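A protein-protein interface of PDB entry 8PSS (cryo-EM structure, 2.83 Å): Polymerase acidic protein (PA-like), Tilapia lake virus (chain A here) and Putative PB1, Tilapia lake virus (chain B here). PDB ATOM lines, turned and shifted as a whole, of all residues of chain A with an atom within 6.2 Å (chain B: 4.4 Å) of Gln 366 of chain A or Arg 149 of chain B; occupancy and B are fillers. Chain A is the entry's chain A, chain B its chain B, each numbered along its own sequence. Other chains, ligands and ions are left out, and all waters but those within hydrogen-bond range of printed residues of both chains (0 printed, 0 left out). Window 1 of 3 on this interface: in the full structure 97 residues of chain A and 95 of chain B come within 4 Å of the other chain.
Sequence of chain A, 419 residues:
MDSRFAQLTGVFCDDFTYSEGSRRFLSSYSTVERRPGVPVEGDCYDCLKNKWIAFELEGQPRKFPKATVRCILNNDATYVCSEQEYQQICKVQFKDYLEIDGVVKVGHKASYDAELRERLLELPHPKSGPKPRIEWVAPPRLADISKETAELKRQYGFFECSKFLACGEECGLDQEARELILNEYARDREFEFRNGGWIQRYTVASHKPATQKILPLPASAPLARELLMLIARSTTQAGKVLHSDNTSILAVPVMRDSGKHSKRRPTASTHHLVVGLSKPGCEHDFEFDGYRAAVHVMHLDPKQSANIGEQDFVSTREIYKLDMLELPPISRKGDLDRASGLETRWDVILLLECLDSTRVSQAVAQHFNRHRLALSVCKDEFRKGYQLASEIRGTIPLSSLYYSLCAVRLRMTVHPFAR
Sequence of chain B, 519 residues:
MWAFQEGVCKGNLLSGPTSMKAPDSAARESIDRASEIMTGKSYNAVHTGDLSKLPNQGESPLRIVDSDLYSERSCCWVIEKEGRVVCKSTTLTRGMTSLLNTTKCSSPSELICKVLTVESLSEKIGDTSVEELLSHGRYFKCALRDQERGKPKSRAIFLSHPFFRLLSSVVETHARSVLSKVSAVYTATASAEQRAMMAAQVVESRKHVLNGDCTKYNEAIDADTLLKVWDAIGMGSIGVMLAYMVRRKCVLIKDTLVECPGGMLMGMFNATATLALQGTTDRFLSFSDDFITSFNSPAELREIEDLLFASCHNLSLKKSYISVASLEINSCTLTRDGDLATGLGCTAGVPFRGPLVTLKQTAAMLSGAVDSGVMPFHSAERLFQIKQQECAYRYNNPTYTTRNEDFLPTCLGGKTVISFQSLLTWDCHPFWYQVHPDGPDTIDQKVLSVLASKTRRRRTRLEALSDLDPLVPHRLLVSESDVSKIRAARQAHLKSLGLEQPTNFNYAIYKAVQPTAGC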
ATOM      1  N   SER A 361       8.419  28.276 -25.789  1.00  0.00           N
ATOM      2  CA  SER A 361       8.224  27.214 -24.812  1.00  0.00           C
ATOM      3  C   SER A 361       7.148  27.584 -23.803  1.00  0.00           C
ATOM      4  O   SER A 361       6.442  26.704 -23.306  1.00  0.00           O
ATOM      5  CB  SER A 361       9.541  26.911 -24.100  1.00  0.00           C
ATOM      6  OG  SER A 361       9.761  27.815 -23.032  1.00  0.00           O
ATOM      7  N   GLN A 362       6.998  28.873 -23.494  1.00  0.00           N
ATOM      8  CA  GLN A 362       5.948  29.288 -22.569  1.00  0.00           C
ATOM      9  C   GLN A 362       4.564  29.078 -23.172  1.00  0.00           C
ATOM     10  O   GLN A 362       3.639  28.636 -22.478  1.00  0.00           O
ATOM     11  CB  GLN A 362       6.148  30.750 -22.176  1.00  0.00           C
ATOM     12  CG  GLN A 362       7.372  30.977 -21.310  1.00  0.00           C
ATOM     13  CD  GLN A 362       7.672  32.442 -21.094  1.00  0.00           C
ATOM     14  OE1 GLN A 362       7.190  33.301 -21.830  1.00  0.00           O
ATOM     15  NE2 GLN A 362       8.472  32.737 -20.079  1.00  0.00           N
ATOM     16  N   ALA A 363       4.397  29.393 -24.458  1.00  0.00           N
ATOM     17  CA  ALA A 363       3.127  29.117 -25.120  1.00  0.00           C
ATOM     18  C   ALA A 363       2.830  27.625 -25.125  1.00  0.00           C
ATOM     19  O   ALA A 363       1.698  27.201 -24.849  1.00  0.00           O
ATOM     20  CB  ALA A 363       3.151  29.662 -26.547  1.00  0.00           C
ATOM     21  N   VAL A 364       3.841  26.808 -25.432  1.00  0.00           N
ATOM     22  CA  VAL A 364       3.640  25.362 -25.424  1.00  0.00           C
ATOM     23  C   VAL A 364       3.267  24.888 -24.025  1.00  0.00           C
ATOM     24  O   VAL A 364       2.410  24.015 -23.861  1.00  0.00           O
ATOM     25  CB  VAL A 364       4.893  24.641 -25.952  1.00  0.00           C
ATOM     26  CG1 VAL A 364       4.689  23.136 -25.925  1.00  0.00           C
ATOM     27  CG2 VAL A 364       5.220  25.108 -27.359  1.00  0.00           C
ATOM     28  N   ALA A 365       3.905  25.452 -22.998  1.00  0.00           N
ATOM     29  CA  ALA A 365       3.612  25.051 -21.625  1.00  0.00           C
ATOM     30  C   ALA A 365       2.189  25.419 -21.230  1.00  0.00           C
ATOM     31  O   ALA A 365       1.504  24.642 -20.557  1.00  0.00           O
ATOM     32  CB  ALA A 365       4.614  25.697 -20.670  1.00  0.00           C
ATOM     33  N   GLN A 366       1.731  26.609 -21.621  1.00  0.00           N
ATOM     34  CA  GLN A 366       0.358  26.999 -21.318  1.00  0.00           C
ATOM     35  C   GLN A 366      -0.637  26.076 -22.010  1.00  0.00           C
ATOM     36  O   GLN A 366      -1.619  25.627 -21.398  1.00  0.00           O
ATOM     37  CB  GLN A 366       0.124  28.450 -21.731  1.00  0.00           C
ATOM     38  CG  GLN A 366       0.769  29.461 -20.803  1.00  0.00           C
ATOM     39  CD  GLN A 366       0.701  30.873 -21.341  1.00  0.00           C
ATOM     40  OE1 GLN A 366      -0.053  31.161 -22.268  1.00  0.00           O
ATOM     41  NE2 GLN A 366       1.496  31.764 -20.761  1.00  0.00           N
ATOM     42  N   HIS A 367      -0.396  25.769 -23.286  1.00  0.00           N
ATOM     43  CA  HIS A 367      -1.303  24.869 -23.989  1.00  0.00           C
ATOM     44  C   HIS A 367      -1.273  23.474 -23.380  1.00  0.00           C
ATOM     45  O   HIS A 367      -2.299  22.792 -23.325  1.00  0.00           O
ATOM     46  CB  HIS A 367      -0.959  24.815 -25.474  1.00  0.00           C
ATOM     47  CG  HIS A 367      -2.125  24.461 -26.344  1.00  0.00           C
ATOM     48  ND1 HIS A 367      -3.314  25.158 -26.310  1.00  0.00           N
ATOM     49  CD2 HIS A 367      -2.291  23.480 -27.260  1.00  0.00           C
ATOM     50  CE1 HIS A 367      -4.159  24.625 -27.172  1.00  0.00           C
ATOM     51  NE2 HIS A 367      -3.563  23.606 -27.763  1.00  0.00           N
ATOM     52  N   PHE A 368      -0.106  23.033 -22.908  1.00  0.00           N
ATOM     53  CA  PHE A 368      -0.015  21.720 -22.278  1.00  0.00           C
ATOM     54  C   PHE A 368      -0.733  21.702 -20.934  1.00  0.00           C
ATOM     55  O   PHE A 368      -1.318  20.684 -20.552  1.00  0.00           O
ATOM     56  CB  PHE A 368       1.451  21.323 -22.113  1.00  0.00           C
ATOM     57  CG  PHE A 368       1.647  19.914 -21.639  1.00  0.00           C
ATOM     58  CD1 PHE A 368       0.996  18.862 -22.259  1.00  0.00           C
ATOM     59  CD2 PHE A 368       2.488  19.639 -20.576  1.00  0.00           C
ATOM     60  CE1 PHE A 368       1.176  17.566 -21.825  1.00  0.00           C
ATOM     61  CE2 PHE A 368       2.674  18.344 -20.139  1.00  0.00           C
ATOM     62  CZ  PHE A 368       2.016  17.308 -20.764  1.00  0.00           C
ATOM     63  N   ASN A 369      -0.691  22.812 -20.198  1.00  0.00           N
ATOM     64  CA  ASN A 369      -1.481  22.910 -18.975  1.00  0.00           C
ATOM     65  C   ASN A 369      -2.966  22.794 -19.283  1.00  0.00           C
ATOM     66  O   ASN A 369      -3.703  22.069 -18.598  1.00  0.00           O
ATOM     67  CB  ASN A 369      -1.182  24.229 -18.263  1.00  0.00           C
ATOM     68  CG  ASN A 369      -1.652  24.232 -16.824  1.00  0.00           C
ATOM     69  OD1 ASN A 369      -1.315  23.338 -16.049  1.00  0.00           O
ATOM     70  ND2 ASN A 369      -2.435  25.239 -16.460  1.00  0.00           N
ATOM     71  N   ARG A 370      -3.424  23.492 -20.325  1.00  0.00           N
ATOM     72  CA  ARG A 370      -4.814  23.348 -20.746  1.00  0.00           C
ATOM     73  C   ARG A 370      -5.122  21.901 -21.114  1.00  0.00           C
ATOM     74  O   ARG A 370      -6.172  21.364 -20.746  1.00  0.00           O
ATOM     75  CB  ARG A 370      -5.104  24.270 -21.930  1.00  0.00           C
ATOM     76  CG  ARG A 370      -5.345  25.719 -21.553  1.00  0.00           C
ATOM     77  CD  ARG A 370      -5.845  26.518 -22.743  1.00  0.00           C
ATOM     78  NE  ARG A 370      -4.770  26.876 -23.660  1.00  0.00           N
ATOM     79  CZ  ARG A 370      -4.028  27.972 -23.564  1.00  0.00           C
ATOM     80  NH1 ARG A 370      -4.214  28.851 -22.594  1.00  0.00           N
ATOM     81  NH2 ARG A 370      -3.075  28.189 -24.464  1.00  0.00           N
ATOM     82  N   HIS A 371      -4.208  21.257 -21.841  1.00  0.00           N
ATOM     83  CA  HIS A 371      -4.377  19.858 -22.221  1.00  0.00           C
ATOM     84  C   HIS A 371      -4.548  18.975 -20.992  1.00  0.00           C
ATOM     85  O   HIS A 371      -5.435  18.116 -20.946  1.00  0.00           O
ATOM     86  CB  HIS A 371      -3.163  19.419 -23.046  1.00  0.00           C
ATOM     87  CG  HIS A 371      -3.291  18.065 -23.677  1.00  0.00           C
ATOM     88  ND1 HIS A 371      -4.040  17.044 -23.135  1.00  0.00           N
ATOM     89  CD2 HIS A 371      -2.738  17.563 -24.807  1.00  0.00           C
ATOM     90  CE1 HIS A 371      -3.950  15.976 -23.907  1.00  0.00           C
ATOM     91  NE2 HIS A 371      -3.167  16.265 -24.929  1.00  0.00           N
ATOM     92  N   LYS B  10       2.380  26.747 -15.410  1.00  0.00           N
ATOM     93  CA  LYS B  10       2.230  27.531 -16.627  1.00  0.00           C
ATOM     94  C   LYS B  10       3.561  27.861 -17.289  1.00  0.00           C
ATOM     95  O   LYS B  10       3.569  28.513 -18.337  1.00  0.00           O
ATOM     96  CB  LYS B  10       1.478  28.830 -16.326  1.00  0.00           C
ATOM     97  CG  LYS B  10       0.115  28.625 -15.691  1.00  0.00           C
ATOM     98  CD  LYS B  10      -0.959  29.415 -16.422  1.00  0.00           C
ATOM     99  CE  LYS B  10      -2.355  29.075 -15.921  1.00  0.00           C
ATOM    100  NZ  LYS B  10      -2.358  28.542 -14.530  1.00  0.00           N
ATOM    101  N   ASN B  12       5.998  29.874 -16.101  1.00  0.00           N
ATOM    102  CA  ASN B  12       6.191  31.308 -15.937  1.00  0.00           C
ATOM    103  C   ASN B  12       7.532  31.659 -15.307  1.00  0.00           C
ATOM    104  O   ASN B  12       7.769  32.832 -15.002  1.00  0.00           O
ATOM    105  CB  ASN B  12       5.063  31.891 -15.079  1.00  0.00           C
ATOM    106  CG  ASN B  12       3.794  32.134 -15.870  1.00  0.00           C
ATOM    107  OD1 ASN B  12       3.736  31.875 -17.070  1.00  0.00           O
ATOM    108  ND2 ASN B  12       2.767  32.632 -15.195  1.00  0.00           N
ATOM    109  N   LEU B  14      10.444  31.958 -16.441  1.00  0.00           N
ATOM    110  CA  LEU B  14      11.278  32.831 -17.253  1.00  0.00           C
ATOM    111  C   LEU B  14      10.517  34.092 -17.640  1.00  0.00           C
ATOM    112  O   LEU B  14       9.291  34.172 -17.519  1.00  0.00           O
ATOM    113  CB  LEU B  14      11.760  32.107 -18.514  1.00  0.00           C
ATOM    114  CG  LEU B  14      12.620  30.861 -18.302  1.00  0.00           C
ATOM    115  CD1 LEU B  14      12.986  30.243 -19.639  1.00  0.00           C
ATOM    116  CD2 LEU B  14      13.870  31.188 -17.502  1.00  0.00           C
ATOM    117  N   SER B  15      11.264  35.086 -18.107  1.00  0.00           N
ATOM    118  CA  SER B  15      10.663  36.330 -18.554  1.00  0.00           C
ATOM    119  C   SER B  15       9.909  36.120 -19.863  1.00  0.00           C
ATOM    120  O   SER B  15      10.104  35.131 -20.575  1.00  0.00           O
ATOM    121  CB  SER B  15      11.732  37.409 -18.735  1.00  0.00           C
ATOM    122  OG  SER B  15      12.400  37.673 -17.516  1.00  0.00           O
ATOM    123  N   GLY B  16       9.038  37.069 -20.176  1.00  0.00           N
ATOM    124  CA  GLY B  16       8.254  37.006 -21.387  1.00  0.00           C
ATOM    125  C   GLY B  16       9.068  37.367 -22.607  1.00  0.00           C
ATOM    126  O   GLY B  16      10.208  37.847 -22.528  1.00  0.00           O
ATOM    127  N   PRO B  17       8.479  37.138 -23.778  1.00  0.00           N
ATOM    128  CA  PRO B  17       9.196  37.415 -25.027  1.00  0.00           C
ATOM    129  C   PRO B  17       9.437  38.901 -25.231  1.00  0.00           C
ATOM    130  O   PRO B  17       8.683  39.752 -24.754  1.00  0.00           O
ATOM    131  CB  PRO B  17       8.262  36.853 -26.103  1.00  0.00           C
ATOM    132  CG  PRO B  17       6.916  36.853 -25.481  1.00  0.00           C
ATOM    133  CD  PRO B  17       7.122  36.622 -24.017  1.00  0.00           C
ATOM    134  N   GLN B 147       7.131  41.242 -23.628  1.00  0.00           N
ATOM    135  CA  GLN B 147       7.191  40.587 -22.324  1.00  0.00           C
ATOM    136  C   GLN B 147       5.844  40.013 -21.905  1.00  0.00           C
ATOM    137  O   GLN B 147       5.563  39.891 -20.708  1.00  0.00           O
ATOM    138  CB  GLN B 147       7.711  41.545 -21.248  1.00  0.00           C
ATOM    139  CG  GLN B 147       9.104  42.085 -21.523  1.00  0.00           C
ATOM    140  CD  GLN B 147      10.165  41.425 -20.667  1.00  0.00           C
ATOM    141  OE1 GLN B 147      10.155  41.546 -19.442  1.00  0.00           O
ATOM    142  NE2 GLN B 147      11.089  40.719 -21.309  1.00  0.00           N
ATOM    143  N   GLU B 148       5.001  39.654 -22.869  1.00  0.00           N
ATOM    144  CA  GLU B 148       3.703  39.050 -22.591  1.00  0.00           C
ATOM    145  C   GLU B 148       3.843  37.538 -22.726  1.00  0.00           C
ATOM    146  O   GLU B 148       3.954  37.015 -23.839  1.00  0.00           O
ATOM    147  CB  GLU B 148       2.642  39.598 -23.541  1.00  0.00           C
ATOM    148  CG  GLU B 148       1.341  39.979 -22.862  1.00  0.00           C
ATOM    149  CD  GLU B 148       0.286  40.446 -23.845  1.00  0.00           C
ATOM    150  OE1 GLU B 148       0.510  40.311 -25.066  1.00  0.00           O
ATOM    151  OE2 GLU B 148      -0.766  40.950 -23.398  1.00  0.00           O
ATOM    152  N   ARG B 149       3.841  36.841 -21.593  1.00  0.00           N
ATOM    153  CA  ARG B 149       4.095  35.407 -21.595  1.00  0.00           C
ATOM    154  C   ARG B 149       3.072  34.674 -22.453  1.00  0.00           C
ATOM    155  O   ARG B 149       1.873  34.962 -22.406  1.00  0.00           O
ATOM    156  CB  ARG B 149       4.061  34.867 -20.167  1.00  0.00           C
ATOM    157  CG  ARG B 149       5.433  34.725 -19.533  1.00  0.00           C
ATOM    158  CD  ARG B 149       5.352  34.684 -18.019  1.00  0.00           C
ATOM    159  NE  ARG B 149       6.575  35.175 -17.397  1.00  0.00           N
ATOM    160  CZ  ARG B 149       6.623  35.926 -16.304  1.00  0.00           C
ATOM    161  NH1 ARG B 149       5.524  36.295 -15.665  1.00  0.00           N
ATOM    162  NH2 ARG B 149       7.805  36.314 -15.837  1.00  0.00           N
ATOM    163  N   GLY B 150       3.555  33.714 -23.237  1.00  0.00           N
ATOM    164  CA  GLY B 150       2.697  32.898 -24.069  1.00  0.00           C
ATOM    165  C   GLY B 150       2.346  33.483 -25.417  1.00  0.00           C
ATOM    166  O   GLY B 150       1.520  32.898 -26.127  1.00  0.00           O
ATOM    167  N   LYS B 151       2.939  34.613 -25.794  1.00  0.00           N
ATOM    168  CA  LYS B 151       2.674  35.266 -27.076  1.00  0.00           C
ATOM    169  C   LYS B 151       4.005  35.549 -27.757  1.00  0.00           C
ATOM    170  O   LYS B 151       4.543  36.660 -27.659  1.00  0.00           O
ATOM    171  CB  LYS B 151       1.864  36.548 -26.886  1.00  0.00           C
ATOM    172  CG  LYS B 151       0.361  36.321 -26.835  1.00  0.00           C
ATOM    173  CD  LYS B 151      -0.231  36.753 -25.503  1.00  0.00           C
ATOM    174  CE  LYS B 151      -1.592  36.115 -25.273  1.00  0.00           C
ATOM    175  NZ  LYS B 151      -1.483  34.665 -24.957  1.00  0.00           N
ATOM    176  N   ALA B 348       6.229  33.036 -10.805  1.00  0.00           N
ATOM    177  CA  ALA B 348       7.066  33.650 -11.824  1.00  0.00           C
ATOM    178  C   ALA B 348       8.451  33.928 -11.261  1.00  0.00           C
ATOM    179  O   ALA B 348       8.589  34.369 -10.116  1.00  0.00           O
ATOM    180  CB  ALA B 348       6.440  34.950 -12.333  1.00  0.00           C
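NE2 of Gln 362 of chain A sits at hydrogen-bond distance from O of Ser 15 of chain B, at 2.9 Å. The side-chain amide nitrogen (NE2) of Gln 362 of chain A sits at hydrogen-bond distance from the backbone carbonyl oxygen (O) of Leu 14 of chain B (3.0 Å).
O of Pro 17 of chain B sits at hydrogen-bond distance from N of Gln 147 of chain B, 2.4 Å away. The guanidinium group (NE) of Arg 149 of chain B lies within hydrogen-bond range of the backbone carbonyl oxygen (O) of Leu 14 of chain B (2.9 Å). NE2 of Gln 147 of chain B lies within hydrogen-bond range of O of Gly 16 of chain B (3.2 Å).
Among the printed residues, merely in contact across the chains: Gln 362 of chain A with Gly 16 of chain B (3.9 Å), Gln 362 of chain A with Pro 17 of chain B (3.98 Å), Gln 362 of chain A with Arg 149 of chain B (3.2 Å), Gln 362 of chain A with Gly 150 of chain B (3.9 Å), Ala 363 of chain A with Gly 150 of chain B (3.6 Å), Ala 365 of chain A with Lys 10 of chain B (3.8 Å), Gln 366 of chain A with Lys 10 of chain B (3.8 Å), Gln 366 of chain A with Arg 149 of chain B (3.6 Å), Gln 366 of chain A with Gly 150 of chain B (3.7 Å) and Asn 369 of chain A with Lys 10 of chain B (3.8 Å).
Of the printed residues of chain B, Ala 365 of chain A touches Lys 10 (3.8 Å). Of chain B, only Lys 10 (3.8 Å), Arg 149 (3.6 Å) and Gly 150 (3.7 Å) come within 4 Å of Gln 366 of chain A. Phe 368 of chain A touches none of the printed residues of chain B. Of the printed residues of chain A, Ser 15 of chain B touches Gln 362 (2.9 Å). Of chain A, only Gln 362 and Gln 366 come within 4 Å of Arg 149 of chain B.
Of the 12 printed residues of chain B, 7 touch a printed residue of chain A. Hydrophobic or aromatic side chains of chain B within 4 Å of the printed part of chain A: Leu 14 and Pro 17. Printed residues of chain A that touch a printed residue of chain B: Gln 362, Ala 363, Ala 365, Gln 366 and Asn 369. Hydrophobic or aromatic side chains of chain A within 4 Å of the printed part of chain B: Ala 363 and Ala 365. Along chain A the printed residues that touch a printed residue of chain B span positions 362 to 369. Among the printed residues, 12 pairs touch across the chains. Among the printed residues, no Asp or Glu carboxylate lies within 4 Å of a Lys or Arg side-chain nitrogen of the other chain.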
